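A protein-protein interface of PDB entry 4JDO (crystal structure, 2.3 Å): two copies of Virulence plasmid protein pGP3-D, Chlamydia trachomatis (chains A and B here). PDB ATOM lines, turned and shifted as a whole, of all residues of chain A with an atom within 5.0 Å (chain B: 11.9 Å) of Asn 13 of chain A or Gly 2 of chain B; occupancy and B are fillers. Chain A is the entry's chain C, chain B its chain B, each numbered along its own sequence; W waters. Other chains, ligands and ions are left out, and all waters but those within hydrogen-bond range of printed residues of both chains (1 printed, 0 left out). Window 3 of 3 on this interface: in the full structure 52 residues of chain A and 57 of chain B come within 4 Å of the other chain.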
ATOM      1  N   PHE A   6       3.772   1.933  25.125  1.00  0.00           N
ATOM      2  CA  PHE A   6       3.591   3.370  25.110  1.00  0.00           C
ATOM      3  C   PHE A   6       3.388   3.799  23.654  1.00  0.00           C
ATOM      4  O   PHE A   6       3.918   3.168  22.740  1.00  0.00           O
ATOM      5  CB  PHE A   6       4.792   4.065  25.758  1.00  0.00           C
ATOM      6  CG  PHE A   6       5.010   3.676  27.206  1.00  0.00           C
ATOM      7  CD1 PHE A   6       5.687   2.512  27.541  1.00  0.00           C
ATOM      8  CD2 PHE A   6       4.515   4.468  28.237  1.00  0.00           C
ATOM      9  CE1 PHE A   6       5.876   2.158  28.874  1.00  0.00           C
ATOM     10  CE2 PHE A   6       4.709   4.117  29.568  1.00  0.00           C
ATOM     11  CZ  PHE A   6       5.384   2.965  29.887  1.00  0.00           C
ATOM     12  N   TYR A   7       2.581   4.833  23.436  1.00  0.00           N
ATOM     13  CA  TYR A   7       2.319   5.319  22.083  1.00  0.00           C
ATOM     14  C   TYR A   7       1.930   6.792  22.093  1.00  0.00           C
ATOM     15  O   TYR A   7       1.361   7.291  23.069  1.00  0.00           O
ATOM     16  CB  TYR A   7       1.240   4.482  21.377  1.00  0.00           C
ATOM     17  CG  TYR A   7      -0.193   4.909  21.642  1.00  0.00           C
ATOM     18  CD1 TYR A   7      -0.679   5.029  22.933  1.00  0.00           C
ATOM     19  CD2 TYR A   7      -1.059   5.200  20.590  1.00  0.00           C
ATOM     20  CE1 TYR A   7      -1.986   5.425  23.176  1.00  0.00           C
ATOM     21  CE2 TYR A   7      -2.370   5.591  20.821  1.00  0.00           C
ATOM     22  CZ  TYR A   7      -2.827   5.703  22.122  1.00  0.00           C
ATOM     23  OH  TYR A   7      -4.129   6.083  22.385  1.00  0.00           O
ATOM     24  N   LEU A   8       2.232   7.483  21.000  1.00  0.00           N
ATOM     25  CA  LEU A   8       1.828   8.874  20.862  1.00  0.00           C
ATOM     26  C   LEU A   8       0.412   8.995  20.292  1.00  0.00           C
ATOM     27  O   LEU A   8       0.138   8.587  19.171  1.00  0.00           O
ATOM     28  CB  LEU A   8       2.833   9.644  20.017  1.00  0.00           C
ATOM     29  CG  LEU A   8       4.235   9.832  20.615  1.00  0.00           C
ATOM     30  CD1 LEU A   8       5.240  10.229  19.538  1.00  0.00           C
ATOM     31  CD2 LEU A   8       4.223  10.864  21.744  1.00  0.00           C
ATOM     32  N   THR A  11      -0.140  14.585  20.532  1.00  0.00           N
ATOM     33  CA  THR A  11       1.152  14.887  21.155  1.00  0.00           C
ATOM     34  C   THR A  11       1.330  14.214  22.521  1.00  0.00           C
ATOM     35  O   THR A  11       2.396  14.299  23.130  1.00  0.00           O
ATOM     36  CB  THR A  11       1.377  16.404  21.319  1.00  0.00           C
ATOM     37  OG1 THR A  11       0.353  16.946  22.158  1.00  0.00           O
ATOM     38  CG2 THR A  11       1.342  17.088  19.963  1.00  0.00           C
ATOM     39  N   GLU A  12       0.287  13.553  23.004  1.00  0.00           N
ATOM     40  CA  GLU A  12       0.336  12.961  24.335  1.00  0.00           C
ATOM     41  C   GLU A  12       0.992  11.581  24.278  1.00  0.00           C
ATOM     42  O   GLU A  12       0.504  10.690  23.585  1.00  0.00           O
ATOM     43  CB  GLU A  12      -1.080  12.852  24.919  1.00  0.00           C
ATOM     44  CG  GLU A  12      -1.910  14.136  24.819  1.00  0.00           C
ATOM     45  CD  GLU A  12      -3.418  13.874  24.772  1.00  0.00           C
ATOM     46  OE1 GLU A  12      -3.949  13.238  25.711  1.00  0.00           O
ATOM     47  OE2 GLU A  12      -4.072  14.314  23.792  1.00  0.00           O
ATOM     48  N   ASN A  13       2.100  11.420  24.998  1.00  0.00           N
ATOM     49  CA  ASN A  13       2.726  10.116  25.212  1.00  0.00           C
ATOM     50  C   ASN A  13       1.910   9.307  26.223  1.00  0.00           C
ATOM     51  O   ASN A  13       2.001   9.543  27.438  1.00  0.00           O
ATOM     52  CB  ASN A  13       4.147  10.307  25.746  1.00  0.00           C
ATOM     53  CG  ASN A  13       5.039   9.082  25.540  1.00  0.00           C
ATOM     54  OD1 ASN A  13       4.573   7.938  25.451  1.00  0.00           O
ATOM     55  ND2 ASN A  13       6.342   9.327  25.479  1.00  0.00           N
ATOM     56  N   CYS A  14       1.110   8.366  25.726  1.00  0.00           N
ATOM     57  CA  CYS A  14       0.246   7.576  26.595  1.00  0.00           C
ATOM     58  C   CYS A  14       0.751   6.170  26.838  1.00  0.00           C
ATOM     59  O   CYS A  14       1.426   5.585  26.008  1.00  0.00           O
ATOM     60  CB  CYS A  14      -1.161   7.476  26.013  1.00  0.00           C
ATOM     61  SG  CYS A  14      -1.792   9.051  25.512  1.00  0.00           S
ATOM     62  N   VAL A  15       0.404   5.638  27.997  1.00  0.00           N
ATOM     63  CA  VAL A  15       0.592   4.243  28.277  1.00  0.00           C
ATOM     64  C   VAL A  15      -0.681   3.573  27.776  1.00  0.00           C
ATOM     65  O   VAL A  15      -1.768   4.167  27.838  1.00  0.00           O
ATOM     66  CB  VAL A  15       0.798   4.008  29.810  1.00  0.00           C
ATOM     67  CG1 VAL A  15      -0.434   4.450  30.606  1.00  0.00           C
ATOM     68  CG2 VAL A  15       1.158   2.555  30.110  1.00  0.00           C
ATOM     69  N   MET B   1       4.007  18.352  25.956  1.00  0.00           N
ATOM     70  CA  MET B   1       4.788  17.508  26.859  1.00  0.00           C
ATOM     71  C   MET B   1       5.387  16.306  26.099  1.00  0.00           C
ATOM     72  O   MET B   1       6.159  16.505  25.167  1.00  0.00           O
ATOM     73  CB  MET B   1       3.943  17.096  28.072  1.00  0.00           C
ATOM     74  CG  MET B   1       2.605  16.411  27.752  1.00  0.00           C
ATOM     75  SD  MET B   1       1.033  17.431  27.170  1.00  0.00           S
ATOM     76  CE  MET B   1       0.747  18.557  28.758  1.00  0.00           C
ATOM     77  N   GLY B   2       5.064  15.075  26.485  1.00  0.00           N
ATOM     78  CA  GLY B   2       5.400  13.934  25.648  1.00  0.00           C
ATOM     79  C   GLY B   2       6.294  12.849  26.219  1.00  0.00           C
ATOM     80  O   GLY B   2       6.798  12.022  25.459  1.00  0.00           O
ATOM     81  N   ASN B   3       6.479  12.826  27.539  1.00  0.00           N
ATOM     82  CA  ASN B   3       7.342  11.815  28.167  1.00  0.00           C
ATOM     83  C   ASN B   3       6.580  10.753  28.942  1.00  0.00           C
ATOM     84  O   ASN B   3       5.517  11.034  29.492  1.00  0.00           O
ATOM     85  CB  ASN B   3       8.372  12.485  29.064  1.00  0.00           C
ATOM     86  CG  ASN B   3       9.093  13.598  28.345  1.00  0.00           C
ATOM     87  OD1 ASN B   3       9.446  13.457  27.172  1.00  0.00           O
ATOM     88  ND2 ASN B   3       9.284  14.725  29.024  1.00  0.00           N
ATOM     89  N   SER B   4       7.126   9.537  28.978  1.00  0.00           N
ATOM     90  CA  SER B   4       6.467   8.417  29.634  1.00  0.00           C
ATOM     91  C   SER B   4       7.425   7.274  29.941  1.00  0.00           C
ATOM     92  O   SER B   4       8.504   7.184  29.364  1.00  0.00           O
ATOM     93  CB  SER B   4       5.308   7.916  28.786  1.00  0.00           C
ATOM     94  OG  SER B   4       5.789   7.155  27.712  1.00  0.00           O
ATOM     95  N   GLY B   5       7.024   6.403  30.861  1.00  0.00           N
ATOM     96  CA  GLY B   5       7.848   5.282  31.284  1.00  0.00           C
ATOM     97  C   GLY B   5       7.566   4.870  32.716  1.00  0.00           C
ATOM     98  O   GLY B   5       6.436   4.937  33.171  1.00  0.00           O
ATOM     99  N   PHE B   6       8.598   4.437  33.427  1.00  0.00           N
ATOM    100  CA  PHE B   6       8.474   4.094  34.832  1.00  0.00           C
ATOM    101  C   PHE B   6       9.563   4.791  35.612  1.00  0.00           C
ATOM    102  O   PHE B   6      10.704   4.854  35.163  1.00  0.00           O
ATOM    103  CB  PHE B   6       8.619   2.599  35.052  1.00  0.00           C
ATOM    104  CG  PHE B   6       7.614   1.779  34.319  1.00  0.00           C
ATOM    105  CD1 PHE B   6       7.873   1.329  33.029  1.00  0.00           C
ATOM    106  CD2 PHE B   6       6.416   1.443  34.914  1.00  0.00           C
ATOM    107  CE1 PHE B   6       6.949   0.557  32.344  1.00  0.00           C
ATOM    108  CE2 PHE B   6       5.481   0.664  34.234  1.00  0.00           C
ATOM    109  CZ  PHE B   6       5.748   0.221  32.947  1.00  0.00           C
ATOM    110  N   CYS B  14       6.689   3.390  39.833  1.00  0.00           N
ATOM    111  CA  CYS B  14       5.465   3.927  39.235  1.00  0.00           C
ATOM    112  C   CYS B  14       5.505   4.036  37.730  1.00  0.00           C
ATOM    113  O   CYS B  14       6.493   4.488  37.176  1.00  0.00           O
ATOM    114  CB  CYS B  14       5.199   5.340  39.745  1.00  0.00           C
ATOM    115  SG  CYS B  14       4.932   5.456  41.496  1.00  0.00           S
ATOM    116  N   VAL B  15       4.402   3.693  37.072  1.00  0.00           N
ATOM    117  CA  VAL B  15       4.230   4.077  35.691  1.00  0.00           C
ATOM    118  C   VAL B  15       3.847   5.580  35.622  1.00  0.00           C
ATOM    119  O   VAL B  15       3.049   6.070  36.436  1.00  0.00           O
ATOM    120  CB  VAL B  15       3.163   3.206  35.006  1.00  0.00           C
ATOM    121  CG1 VAL B  15       1.786   3.384  35.673  1.00  0.00           C
ATOM    122  CG2 VAL B  15       3.095   3.523  33.528  1.00  0.00           C
ATOM    123  N   PHE B  16       4.431   6.305  34.670  1.00  0.00           N
ATOM    124  CA  PHE B  16       4.054   7.696  34.420  1.00  0.00           C
ATOM    125  C   PHE B  16       3.862   7.930  32.922  1.00  0.00           C
ATOM    126  O   PHE B  16       4.499   7.254  32.093  1.00  0.00           O
ATOM    127  CB  PHE B  16       5.095   8.665  34.993  1.00  0.00           C
ATOM    128  CG  PHE B  16       6.328   8.809  34.138  1.00  0.00           C
ATOM    129  CD1 PHE B  16       7.372   7.889  34.236  1.00  0.00           C
ATOM    130  CD2 PHE B  16       6.452   9.870  33.238  1.00  0.00           C
ATOM    131  CE1 PHE B  16       8.520   8.022  33.456  1.00  0.00           C
ATOM    132  CE2 PHE B  16       7.598  10.010  32.448  1.00  0.00           C
ATOM    133  CZ  PHE B  16       8.629   9.077  32.552  1.00  0.00           C
ATOM    134  N   ALA B  17       2.972   8.869  32.584  1.00  0.00           N
ATOM    135  CA  ALA B  17       2.634   9.189  31.187  1.00  0.00           C
ATOM    136  C   ALA B  17       1.761  10.423  31.149  1.00  0.00           C
ATOM    137  O   ALA B  17       1.306  10.872  32.194  1.00  0.00           O
ATOM    138  CB  ALA B  17       1.905   8.012  30.492  1.00  0.00           C
ATOM    139  N   ASP B  18       1.520  10.957  29.949  1.00  0.00           N
ATOM    140  CA  ASP B  18       0.670  12.139  29.791  1.00  0.00           C
ATOM    141  C   ASP B  18      -0.782  11.755  29.914  1.00  0.00           C
ATOM    142  O   ASP B  18      -1.613  12.557  30.329  1.00  0.00           O
ATOM    143  CB  ASP B  18       0.855  12.802  28.420  1.00  0.00           C
ATOM    144  CG  ASP B  18       2.257  13.284  28.193  1.00  0.00           C
ATOM    145  OD1 ASP B  18       2.908  13.692  29.175  1.00  0.00           O
ATOM    146  OD2 ASP B  18       2.708  13.261  27.027  1.00  0.00           O
ATOM    147  N   ASN B  19      -1.076  10.524  29.510  1.00  0.00           N
ATOM    148  CA  ASN B  19      -2.434  10.006  29.506  1.00  0.00           C
ATOM    149  C   ASN B  19      -2.412   8.469  29.450  1.00  0.00           C
ATOM    150  O   ASN B  19      -1.355   7.852  29.437  1.00  0.00           O
ATOM    151  CB  ASN B  19      -3.247  10.622  28.355  1.00  0.00           C
ATOM    152  CG  ASN B  19      -4.729  10.802  28.706  1.00  0.00           C
ATOM    153  OD1 ASN B  19      -5.329   9.982  29.415  1.00  0.00           O
ATOM    154  ND2 ASN B  19      -5.323  11.871  28.204  1.00  0.00           N
ATOM    155  N   ILE B  20      -3.578   7.852  29.427  1.00  0.00           N
ATOM    156  CA  ILE B  20      -3.661   6.408  29.539  1.00  0.00           C
ATOM    157  C   ILE B  20      -4.824   5.895  28.708  1.00  0.00           C
ATOM    158  O   ILE B  20      -5.897   6.507  28.667  1.00  0.00           O
ATOM    159  CB  ILE B  20      -3.843   5.993  31.012  1.00  0.00           C
ATOM    160  CG1 ILE B  20      -4.070   4.479  31.151  1.00  0.00           C
ATOM    161  CG2 ILE B  20      -4.959   6.834  31.682  1.00  0.00           C
ATOM    162  CD1 ILE B  20      -4.104   3.996  32.600  1.00  0.00           C
ATOM    163  N   LYS B  21      -4.608   4.782  28.024  1.00  0.00           N
ATOM    164  CA  LYS B  21      -5.687   4.141  27.310  1.00  0.00           C
ATOM    165  C   LYS B  21      -5.710   2.657  27.669  1.00  0.00           C
ATOM    166  O   LYS B  21      -4.769   1.930  27.385  1.00  0.00           O
ATOM    167  CB  LYS B  21      -5.509   4.333  25.797  1.00  0.00           C
ATOM    168  CG  LYS B  21      -6.682   3.830  24.982  1.00  0.00           C
ATOM    169  CD  LYS B  21      -6.448   3.969  23.489  1.00  0.00           C
ATOM    170  CE  LYS B  21      -5.476   2.916  22.983  1.00  0.00           C
ATOM    171  NZ  LYS B  21      -5.418   2.922  21.495  1.00  0.00           N
ATOM    172  N   VAL B  22      -6.778   2.196  28.299  1.00  0.00           N
ATOM    173  CA  VAL B  22      -6.846   0.784  28.633  1.00  0.00           C
ATOM    174  C   VAL B  22      -8.142   0.153  28.170  1.00  0.00           C
ATOM    175  O   VAL B  22      -9.166   0.826  28.086  1.00  0.00           O
ATOM    176  CB  VAL B  22      -6.665   0.542  30.145  1.00  0.00           C
ATOM    177  CG1 VAL B  22      -5.194   0.630  30.515  1.00  0.00           C
ATOM    178  CG2 VAL B  22      -7.505   1.537  30.946  1.00  0.00           C
ATOM    179  N   GLU B  27      -9.802   5.873  22.708  1.00  0.00           N
ATOM    180  CA  GLU B  27      -8.966   7.059  22.826  1.00  0.00           C
ATOM    181  C   GLU B  27      -8.565   7.173  24.296  1.00  0.00           C
ATOM    182  O   GLU B  27      -9.192   6.554  25.151  1.00  0.00           O
ATOM    183  CB  GLU B  27      -9.741   8.289  22.359  1.00  0.00           C
ATOM    184  CG  GLU B  27     -11.157   8.342  22.927  1.00  0.00           C
ATOM    185  CD  GLU B  27     -12.063   9.338  22.215  1.00  0.00           C
ATOM    186  OE1 GLU B  27     -11.973   9.455  20.971  1.00  0.00           O
ATOM    187  OE2 GLU B  27     -12.872   9.998  22.906  1.00  0.00           O
ATOM    188  N   PRO B  28      -7.500   7.933  24.591  1.00  0.00           N
ATOM    189  CA  PRO B  28      -7.107   8.200  25.983  1.00  0.00           C
ATOM    190  C   PRO B  28      -8.194   8.930  26.791  1.00  0.00           C
ATOM    191  O   PRO B  28      -9.167   9.437  26.212  1.00  0.00           O
ATOM    192  CB  PRO B  28      -5.870   9.092  25.832  1.00  0.00           C
ATOM    193  CG  PRO B  28      -5.327   8.747  24.474  1.00  0.00           C
ATOM    194  CD  PRO B  28      -6.516   8.453  23.623  1.00  0.00           C
ATOM    195  N   LEU B  29      -8.017   8.969  28.113  1.00  0.00           N
ATOM    196  CA  LEU B  29      -8.952   9.626  29.029  1.00  0.00           C
ATOM    197  C   LEU B  29      -9.309  11.038  28.606  1.00  0.00           C
ATOM    198  O   LEU B  29      -8.443  11.902  28.530  1.00  0.00           O
ATOM    199  CB  LEU B  29      -8.364   9.703  30.433  1.00  0.00           C
ATOM    200  CG  LEU B  29      -8.826   8.703  31.487  1.00  0.00           C
ATOM    201  CD1 LEU B  29      -8.720   9.372  32.835  1.00  0.00           C
ATOM    202  CD2 LEU B  29     -10.244   8.209  31.246  1.00  0.00           C
HETATM  203  O   HOH W   1      -6.048   5.949  19.948  1.00  0.00           O
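Water W1 lies within hydrogen-bond range of OH of Tyr 7 of chain A (3.1 Å) and NZ of Lys 21 of chain B (3.5 Å).
Printed residues of chain A that touch a printed residue of chain B: Phe 6, Tyr 7, Thr 11, Glu 12, Asn 13, Cys 14 and Val 15.
Hydrophobic or aromatic side chains of chain A that line the printed part of chain B: Phe 6, Tyr 7 and Val 15.
Of the 18 printed residues of chain B, 11 touch a printed residue of chain A.
Hydrophobic or aromatic side chains of chain B that line the printed part of chain A: Phe 6, Ala 17, Ile 20 and Pro 28.
Ser 4 of chain B touches Phe 6 of chain A (OG to CD2, 3.0 Å).
Gly 5 of chain B touches Phe 6 of chain A (N to CE2, 3.5 Å).
OH of Tyr 7 of chain A touches CD of Pro 28 of chain B, at 3.6 Å.
Thr 11 of chain A touches Gly 2 of chain B.
Glu 12 of chain A touches Asp 18 of chain B.
Asn 13 of chain A touches Ala 17 of chain B (O to CB, 3.4 Å).
N of Asn 19 of chain B touches O of Asn 13 of chain A (3.8 Å).
Asn 19 of chain B touches Cys 14 of chain A.
CG of Pro 28 of chain B touches SG of Cys 14 of chain A, at 3.7 Å.
CA of Ile 20 of chain B touches O of Val 15 of chain A, at 3.4 Å.
ND2 of Asn 19 of chain B is in hydrogen-bond range of OE1 of Glu 12 of chain A, at 3.2 Å.
The side-chain carboxylate of Asp 18 of chain B sits at hydrogen-bond distance from the backbone NH of Asn 13 of chain A (2.8 Å).
The backbone NH (N) of Lys 21 of chain B sits at hydrogen-bond distance from the backbone carbonyl oxygen (O) of Val 15 of chain A (2.9 Å).
O of Gly 2 of chain B is in hydrogen-bond range of ND2 of Asn 13 of chain A, 2.7 Å away.
OG of Ser 4 of chain B lies within hydrogen-bond range of OD1 of Asn 13 of chain A.
The backbone carbonyl oxygen (O) of Asn 19 of chain B sits at hydrogen-bond distance from the backbone NH (N) of Val 15 of chain A (3.2 Å).
The side-chain carboxylate of Asp 18 of chain B sits at hydrogen-bond distance from the backbone NH of Gly 2 of chain B, 3.0 Å away.
O of Ile 20 of chain B sits at hydrogen-bond distance from N of Leu 29 of chain B, 3.3 Å away.
SG of Cys 14 of chain A sits at hydrogen-bond distance from O of Glu 12 of chain A, 3.4 Å away.
The backbone carbonyl oxygen of Tyr 7 of chain A sits at hydrogen-bond distance from the backbone NH of Cys 14 of chain A (2.9 Å).
The backbone NH (N) of Phe 16 of chain B is in hydrogen-bond range of the backbone carbonyl oxygen (O) of Gly 5 of chain B, at 2.9 Å.
The side-chain amide nitrogen (ND2) of Asn 19 of chain B lies within hydrogen-bond range of the backbone carbonyl oxygen (O) of Leu 29 of chain B (3.1 Å).
No residue of chain B comes within 4 Å of Leu 8 of chain A.
Of chain B, only Asp 18 (3.6 Å) and Asn 19 (3.2 Å) come within 4 Å of Glu 12 of chain A.
Asn 13 of chain A touches just these residues of chain B: Gly 2, Asn 3, Ser 4, Ala 17, Asp 18 and Asn 19.
Cys 14 of chain A touches two residues of chain B.
Of chain B, only Ala 17, Asn 19, Ile 20 and Lys 21 come within 4 Å of Val 15 of chain A.
Of chain A, only Thr 11 (3.9 Å) and Asn 13 (2.7 Å) come within 4 Å of Gly 2 of chain B.
Of the printed residues of chain A, Ala 17 of chain B touches Asn 13 and Val 15.
Of the printed residues of chain A, Ile 20 of chain B touches Val 15.
Val 22 of chain B touches none of the printed residues of chain A.
Leu 29 of chain B touches none of the printed residues of chain A.
The nearest printed residue of chain A that does not touch Asn 3 of chain B is Thr 11 of chain A (6.2 Å).
Phe 6 of chain B touches its own counterpart, Phe 6 of chain A.
Positions printed for both chains: 6, 14 and 15.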
